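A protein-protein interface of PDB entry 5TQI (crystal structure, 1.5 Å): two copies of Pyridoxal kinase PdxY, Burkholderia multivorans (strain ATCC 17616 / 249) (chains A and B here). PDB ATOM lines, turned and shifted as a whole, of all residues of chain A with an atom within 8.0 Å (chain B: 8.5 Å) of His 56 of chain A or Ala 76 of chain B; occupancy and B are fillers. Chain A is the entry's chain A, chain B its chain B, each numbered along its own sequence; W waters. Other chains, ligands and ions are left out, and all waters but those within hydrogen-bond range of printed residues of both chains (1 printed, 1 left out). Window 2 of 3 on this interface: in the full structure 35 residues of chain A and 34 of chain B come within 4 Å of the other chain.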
ATOM      1  N   SER A  49     -14.176  28.550  31.370  1.00  0.00           N
ATOM      2  CA  SER A  49     -14.422  28.456  29.934  1.00  0.00           C
ATOM      3  C   SER A  49     -14.956  27.077  29.557  1.00  0.00           C
ATOM      4  O   SER A  49     -15.793  26.948  28.651  1.00  0.00           O
ATOM      5  CB  SER A  49     -13.134  28.762  29.161  1.00  0.00           C
ATOM      6  OG  SER A  49     -12.106  27.845  29.506  1.00  0.00           O
ATOM      7  N   ASN A  50     -14.474  26.037  30.230  1.00  0.00           N
ATOM      8  CA  ASN A  50     -14.754  24.644  29.906  1.00  0.00           C
ATOM      9  C   ASN A  50     -14.282  23.825  31.100  1.00  0.00           C
ATOM     10  O   ASN A  50     -13.586  24.342  31.978  1.00  0.00           O
ATOM     11  CB  ASN A  50     -14.028  24.214  28.627  1.00  0.00           C
ATOM     12  CG  ASN A  50     -12.538  24.504  28.682  1.00  0.00           C
ATOM     13  OD1 ASN A  50     -12.076  25.537  28.196  1.00  0.00           O
ATOM     14  ND2 ASN A  50     -11.779  23.594  29.282  1.00  0.00           N
ATOM     15  N   HIS A  51     -14.647  22.544  31.125  1.00  0.00           N
ATOM     16  CA  HIS A  51     -14.282  21.645  32.227  1.00  0.00           C
ATOM     17  C   HIS A  51     -12.774  21.525  32.352  1.00  0.00           C
ATOM     18  O   HIS A  51     -12.054  21.575  31.350  1.00  0.00           O
ATOM     19  CB  HIS A  51     -14.734  20.215  31.939  1.00  0.00           C
ATOM     20  CG  HIS A  51     -16.162  20.090  31.541  1.00  0.00           C
ATOM     21  ND1 HIS A  51     -17.177  20.742  32.202  1.00  0.00           N
ATOM     22  CD2 HIS A  51     -16.749  19.371  30.557  1.00  0.00           C
ATOM     23  CE1 HIS A  51     -18.329  20.445  31.629  1.00  0.00           C
ATOM     24  NE2 HIS A  51     -18.097  19.611  30.632  1.00  0.00           N
ATOM     25  N   MET A  52     -12.299  21.274  33.570  1.00  0.00           N
ATOM     26  CA  MET A  52     -10.872  21.078  33.773  1.00  0.00           C
ATOM     27  C   MET A  52     -10.365  19.786  33.148  1.00  0.00           C
ATOM     28  O   MET A  52      -9.164  19.682  32.873  1.00  0.00           O
ATOM     29  CB  MET A  52     -10.542  21.145  35.262  1.00  0.00           C
ATOM     30  CG  MET A  52     -10.908  22.482  35.875  1.00  0.00           C
ATOM     31  SD  MET A  52     -10.408  22.620  37.595  1.00  0.00           S
ATOM     32  CE  MET A  52     -11.529  21.461  38.373  1.00  0.00           C
ATOM     33  N   GLN A  53     -11.248  18.815  32.886  1.00  0.00           N
ATOM     34  CA  GLN A  53     -10.804  17.554  32.289  1.00  0.00           C
ATOM     35  C   GLN A  53     -10.237  17.728  30.884  1.00  0.00           C
ATOM     36  O   GLN A  53      -9.556  16.820  30.396  1.00  0.00           O
ATOM     37  CB  GLN A  53     -11.931  16.520  32.254  1.00  0.00           C
ATOM     38  CG  GLN A  53     -12.175  15.807  33.562  1.00  0.00           C
ATOM     39  CD  GLN A  53     -12.974  16.635  34.540  1.00  0.00           C
ATOM     40  OE1 GLN A  53     -13.094  17.855  34.395  1.00  0.00           O
ATOM     41  NE2 GLN A  53     -13.548  15.972  35.539  1.00  0.00           N
ATOM     42  N   TYR A  54     -10.510  18.850  30.212  1.00  0.00           N
ATOM     43  CA  TYR A  54      -9.887  19.091  28.915  1.00  0.00           C
ATOM     44  C   TYR A  54      -8.383  19.292  29.031  1.00  0.00           C
ATOM     45  O   TYR A  54      -7.673  19.167  28.028  1.00  0.00           O
ATOM     46  CB  TYR A  54     -10.512  20.305  28.223  1.00  0.00           C
ATOM     47  CG  TYR A  54     -11.870  20.045  27.617  1.00  0.00           C
ATOM     48  CD1 TYR A  54     -11.997  19.490  26.345  1.00  0.00           C
ATOM     49  CD2 TYR A  54     -13.027  20.366  28.312  1.00  0.00           C
ATOM     50  CE1 TYR A  54     -13.248  19.258  25.787  1.00  0.00           C
ATOM     51  CE2 TYR A  54     -14.279  20.138  27.758  1.00  0.00           C
ATOM     52  CZ  TYR A  54     -14.385  19.585  26.498  1.00  0.00           C
ATOM     53  OH  TYR A  54     -15.633  19.363  25.954  1.00  0.00           O
ATOM     54  N   GLY A  55      -7.886  19.605  30.227  1.00  0.00           N
ATOM     55  CA  GLY A  55      -6.477  19.796  30.465  1.00  0.00           C
ATOM     56  C   GLY A  55      -6.049  21.245  30.542  1.00  0.00           C
ATOM     57  O   GLY A  55      -4.983  21.537  31.096  1.00  0.00           O
ATOM     58  N   HIS A  56      -6.848  22.156  29.998  1.00  0.00           N
ATOM     59  CA  HIS A  56      -6.571  23.577  30.104  1.00  0.00           C
ATOM     60  C   HIS A  56      -7.894  24.317  30.085  1.00  0.00           C
ATOM     61  O   HIS A  56      -8.863  23.867  29.469  1.00  0.00           O
ATOM     62  CB  HIS A  56      -5.670  24.077  28.973  1.00  0.00           C
ATOM     63  CG  HIS A  56      -5.892  23.380  27.669  1.00  0.00           C
ATOM     64  ND1 HIS A  56      -6.734  23.873  26.695  1.00  0.00           N
ATOM     65  CD2 HIS A  56      -5.372  22.232  27.171  1.00  0.00           C
ATOM     66  CE1 HIS A  56      -6.726  23.056  25.655  1.00  0.00           C
ATOM     67  NE2 HIS A  56      -5.910  22.052  25.920  1.00  0.00           N
ATOM     68  N   TRP A  57      -7.926  25.452  30.772  1.00  0.00           N
ATOM     69  CA  TRP A  57      -9.147  26.239  30.862  1.00  0.00           C
ATOM     70  C   TRP A  57      -8.770  27.637  31.316  1.00  0.00           C
ATOM     71  O   TRP A  57      -7.662  27.882  31.800  1.00  0.00           O
ATOM     72  CB  TRP A  57     -10.130  25.631  31.867  1.00  0.00           C
ATOM     73  CG  TRP A  57      -9.594  25.641  33.280  1.00  0.00           C
ATOM     74  CD1 TRP A  57      -9.811  26.594  34.239  1.00  0.00           C
ATOM     75  CD2 TRP A  57      -8.737  24.664  33.874  1.00  0.00           C
ATOM     76  NE1 TRP A  57      -9.148  26.260  35.395  1.00  0.00           N
ATOM     77  CE2 TRP A  57      -8.479  25.080  35.197  1.00  0.00           C
ATOM     78  CE3 TRP A  57      -8.163  23.475  33.417  1.00  0.00           C
ATOM     79  CZ2 TRP A  57      -7.673  24.346  36.068  1.00  0.00           C
ATOM     80  CZ3 TRP A  57      -7.368  22.745  34.283  1.00  0.00           C
ATOM     81  CH2 TRP A  57      -7.129  23.185  35.594  1.00  0.00           C
ATOM     82  N   ALA A  58      -9.713  28.554  31.152  1.00  0.00           N
ATOM     83  CA  ALA A  58      -9.634  29.871  31.754  1.00  0.00           C
ATOM     84  C   ALA A  58     -10.766  29.992  32.763  1.00  0.00           C
ATOM     85  O   ALA A  58     -11.781  29.297  32.669  1.00  0.00           O
ATOM     86  CB  ALA A  58      -9.747  30.976  30.699  1.00  0.00           C
ATOM     87  N   GLY A  59     -10.588  30.869  33.745  1.00  0.00           N
ATOM     88  CA  GLY A  59     -11.603  30.989  34.771  1.00  0.00           C
ATOM     89  C   GLY A  59     -11.506  32.273  35.558  1.00  0.00           C
ATOM     90  O   GLY A  59     -10.468  32.945  35.588  1.00  0.00           O
ATOM     91  N   GLN B  69     -10.373  36.393  27.636  1.00  0.00           N
ATOM     92  CA  GLN B  69      -9.611  35.227  28.078  1.00  0.00           C
ATOM     93  C   GLN B  69     -10.506  33.998  28.206  1.00  0.00           C
ATOM     94  O   GLN B  69     -10.079  32.877  27.908  1.00  0.00           O
ATOM     95  CB  GLN B  69      -8.957  35.531  29.425  1.00  0.00           C
ATOM     96  CG  GLN B  69      -7.904  34.537  29.841  1.00  0.00           C
ATOM     97  CD  GLN B  69      -7.425  34.770  31.254  1.00  0.00           C
ATOM     98  OE1 GLN B  69      -7.982  35.595  31.985  1.00  0.00           O
ATOM     99  NE2 GLN B  69      -6.385  34.043  31.652  1.00  0.00           N
ATOM    100  N   LEU B  70     -11.742  34.186  28.674  1.00  0.00           N
ATOM    101  CA  LEU B  70     -12.674  33.067  28.772  1.00  0.00           C
ATOM    102  C   LEU B  70     -12.997  32.496  27.396  1.00  0.00           C
ATOM    103  O   LEU B  70     -13.008  31.275  27.206  1.00  0.00           O
ATOM    104  CB  LEU B  70     -13.946  33.510  29.504  1.00  0.00           C
ATOM    105  CG  LEU B  70     -13.732  33.760  31.005  1.00  0.00           C
ATOM    106  CD1 LEU B  70     -14.882  34.528  31.623  1.00  0.00           C
ATOM    107  CD2 LEU B  70     -13.543  32.447  31.748  1.00  0.00           C
ATOM    108  N   VAL B  71     -13.251  33.361  26.416  1.00  0.00           N
ATOM    109  CA  VAL B  71     -13.518  32.869  25.067  1.00  0.00           C
ATOM    110  C   VAL B  71     -12.265  32.233  24.464  1.00  0.00           C
ATOM    111  O   VAL B  71     -12.352  31.228  23.749  1.00  0.00           O
ATOM    112  CB  VAL B  71     -14.111  33.991  24.197  1.00  0.00           C
ATOM    113  CG1 VAL B  71     -14.286  33.530  22.764  1.00  0.00           C
ATOM    114  CG2 VAL B  71     -15.451  34.402  24.772  1.00  0.00           C
ATOM    115  N   ASP B  72     -11.084  32.785  24.770  1.00  0.00           N
ATOM    116  CA  ASP B  72      -9.831  32.152  24.360  1.00  0.00           C
ATOM    117  C   ASP B  72      -9.745  30.717  24.863  1.00  0.00           C
ATOM    118  O   ASP B  72      -9.169  29.850  24.198  1.00  0.00           O
ATOM    119  CB  ASP B  72      -8.637  32.936  24.913  1.00  0.00           C
ATOM    120  CG  ASP B  72      -8.282  34.157  24.083  1.00  0.00           C
ATOM    121  OD1 ASP B  72      -8.808  34.309  22.960  1.00  0.00           O
ATOM    122  OD2 ASP B  72      -7.455  34.967  24.567  1.00  0.00           O
ATOM    123  N   GLY B  73     -10.279  30.456  26.057  1.00  0.00           N
ATOM    124  CA  GLY B  73     -10.271  29.096  26.572  1.00  0.00           C
ATOM    125  C   GLY B  73     -11.144  28.163  25.753  1.00  0.00           C
ATOM    126  O   GLY B  73     -10.766  27.014  25.496  1.00  0.00           O
ATOM    127  N   ILE B  74     -12.323  28.640  25.335  1.00  0.00           N
ATOM    128  CA  ILE B  74     -13.167  27.856  24.437  1.00  0.00           C
ATOM    129  C   ILE B  74     -12.460  27.622  23.109  1.00  0.00           C
ATOM    130  O   ILE B  74     -12.515  26.525  22.539  1.00  0.00           O
ATOM    131  CB  ILE B  74     -14.533  28.542  24.236  1.00  0.00           C
ATOM    132  CG1 ILE B  74     -15.202  28.825  25.583  1.00  0.00           C
ATOM    133  CG2 ILE B  74     -15.432  27.675  23.379  1.00  0.00           C
ATOM    134  CD1 ILE B  74     -16.474  29.646  25.454  1.00  0.00           C
ATOM    135  N   ALA B  75     -11.795  28.653  22.588  1.00  0.00           N
ATOM    136  CA  ALA B  75     -11.075  28.495  21.332  1.00  0.00           C
ATOM    137  C   ALA B  75      -9.944  27.483  21.476  1.00  0.00           C
ATOM    138  O   ALA B  75      -9.687  26.697  20.558  1.00  0.00           O
ATOM    139  CB  ALA B  75     -10.551  29.853  20.868  1.00  0.00           C
ATOM    140  N   ALA B  76      -9.285  27.461  22.641  1.00  0.00           N
ATOM    141  CA  ALA B  76      -8.113  26.610  22.830  1.00  0.00           C
ATOM    142  C   ALA B  76      -8.459  25.123  22.813  1.00  0.00           C
ATOM    143  O   ALA B  76      -7.596  24.301  22.485  1.00  0.00           O
ATOM    144  CB  ALA B  76      -7.386  26.985  24.123  1.00  0.00           C
ATOM    145  N   ILE B  77      -9.693  24.750  23.164  1.00  0.00           N
ATOM    146  CA  ILE B  77     -10.089  23.345  23.100  1.00  0.00           C
ATOM    147  C   ILE B  77     -10.719  23.039  21.746  1.00  0.00           C
ATOM    148  O   ILE B  77     -11.233  21.937  21.523  1.00  0.00           O
ATOM    149  CB  ILE B  77     -11.006  22.930  24.269  1.00  0.00           C
ATOM    150  CG1 ILE B  77     -12.276  23.775  24.287  1.00  0.00           C
ATOM    151  CG2 ILE B  77     -10.270  23.036  25.597  1.00  0.00           C
ATOM    152  CD1 ILE B  77     -13.361  23.195  25.185  1.00  0.00           C
ATOM    153  N   GLY B  78     -10.690  24.013  20.836  1.00  0.00           N
ATOM    154  CA  GLY B  78     -11.187  23.799  19.492  1.00  0.00           C
ATOM    155  C   GLY B  78     -12.685  23.859  19.329  1.00  0.00           C
ATOM    156  O   GLY B  78     -13.201  23.426  18.293  1.00  0.00           O
ATOM    157  N   ALA B  79     -13.404  24.399  20.308  1.00  0.00           N
ATOM    158  CA  ALA B  79     -14.859  24.367  20.296  1.00  0.00           C
ATOM    159  C   ALA B  79     -15.486  25.592  19.643  1.00  0.00           C
ATOM    160  O   ALA B  79     -16.687  25.571  19.348  1.00  0.00           O
ATOM    161  CB  ALA B  79     -15.389  24.225  21.727  1.00  0.00           C
ATOM    162  N   LEU B  80     -14.712  26.651  19.400  1.00  0.00           N
ATOM    163  CA  LEU B  80     -15.318  27.899  18.948  1.00  0.00           C
ATOM    164  C   LEU B  80     -15.939  27.752  17.563  1.00  0.00           C
ATOM    165  O   LEU B  80     -16.926  28.428  17.251  1.00  0.00           O
ATOM    166  CB  LEU B  80     -14.297  29.038  19.011  1.00  0.00           C
ATOM    167  CG  LEU B  80     -14.815  30.445  19.291  1.00  0.00           C
ATOM    168  CD1 LEU B  80     -15.638  30.497  20.581  1.00  0.00           C
ATOM    169  CD2 LEU B  80     -13.662  31.431  19.348  1.00  0.00           C
ATOM    170  N   MET B 110     -13.409  31.342  13.336  1.00  0.00           N
ATOM    171  CA  MET B 110     -13.503  29.892  13.439  1.00  0.00           C
ATOM    172  C   MET B 110     -14.733  29.335  12.745  1.00  0.00           C
ATOM    173  O   MET B 110     -14.729  28.170  12.333  1.00  0.00           O
ATOM    174  CB  MET B 110     -13.474  29.466  14.910  1.00  0.00           C
ATOM    175  CG  MET B 110     -12.139  29.775  15.597  1.00  0.00           C
ATOM    176  SD  MET B 110     -10.732  28.924  14.850  1.00  0.00           S
ATOM    177  CE  MET B 110     -10.023  30.204  13.801  1.00  0.00           C
HETATM  178  O   HOH W   1      -7.872  31.915  33.711  1.00  0.00           O
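OD1 of Asn 50 of chain A sits close to O of Gly 73 of chain B (3.3 Å).
The side-chain hydroxyl (OG) of Ser 49 of chain A sits at hydrogen-bond distance from the side-chain amide oxygen (OD1) of Asn 50 of chain A (2.7 Å). O of Ile 74 of chain B is in hydrogen-bond range of N of Ala 79 of chain B (3.2 Å). ND2 of Asn 50 of chain A lies within hydrogen-bond range of O of His 56 of chain A (2.9 Å). The backbone NH (N) of Ser 49 of chain A is in hydrogen-bond range of the backbone carbonyl oxygen (O) of Ala 58 of chain A (2.8 Å).
CB of Ser 49 of chain A touches O of Leu 70 of chain B, at 3.2 Å. Gly 73 of chain B touches Ser 49 of chain A. Ile 74 of chain B touches Ser 49 of chain A (CG1 to O, 3.6 Å). Ile 77 of chain B touches Asn 50 of chain A (CD1 to CB, 3.7 Å). CG2 of Ile 77 of chain B touches CB of Tyr 54 of chain A (3.8 Å). CE1 of His 56 of chain A touches O of Ala 76 of chain B, 3.5 Å away. Ile 77 of chain B touches His 56 of chain A (CG2 to CE1, 3.5 Å). Ala 58 of chain A touches Gln 69 of chain B. CD2 of Leu 70 of chain B touches O of Ala 58 of chain A (3.7 Å). Gly 59 of chain A touches Leu 70 of chain B (CA to CD2, 3.9 Å).
Printed residues of chain B within 4 Å of Asn 50 of chain A: Gly 73 and Ile 77. Of the printed residues of chain B, Tyr 54 of chain A touches Ile 77. No residue of chain B comes within 4 Å of Gly 55 of chain A. His 56 of chain A touches just these residues of chain B: Ala 76 (3.5 Å) and Ile 77 (3.5 Å). Of the printed residues of chain A, Leu 70 of chain B touches Ser 49, Ala 58 and Gly 59. Of chain A, only His 56 (3.5 Å) comes within 4 Å of Ala 76 of chain B. The nearest residue of chain A that does not touch Ala 76 of chain B is Asn 50 of chain A (6.4 Å). The nearest printed residue of chain B that does not touch Gly 59 of chain A is Gln 69 of chain B (5.1 Å).
Of the 13 printed residues of chain B, 6 touch a printed residue of chain A. Hydrophobic or aromatic side chains of chain B within 4 Å of the printed part of chain A: Leu 70, Ile 74 and Ile 77. Printed residues of chain A that touch a printed residue of chain B: Ser 49, Asn 50, Tyr 54, His 56, Ala 58 and Gly 59. Along chain A the printed residues that touch a printed residue of chain B span positions 49 to 59.
No position is printed for both chains.
Water W1 lies within hydrogen-bond range of N of Gly 59 of chain A and NE2 of Gln 69 of chain B.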
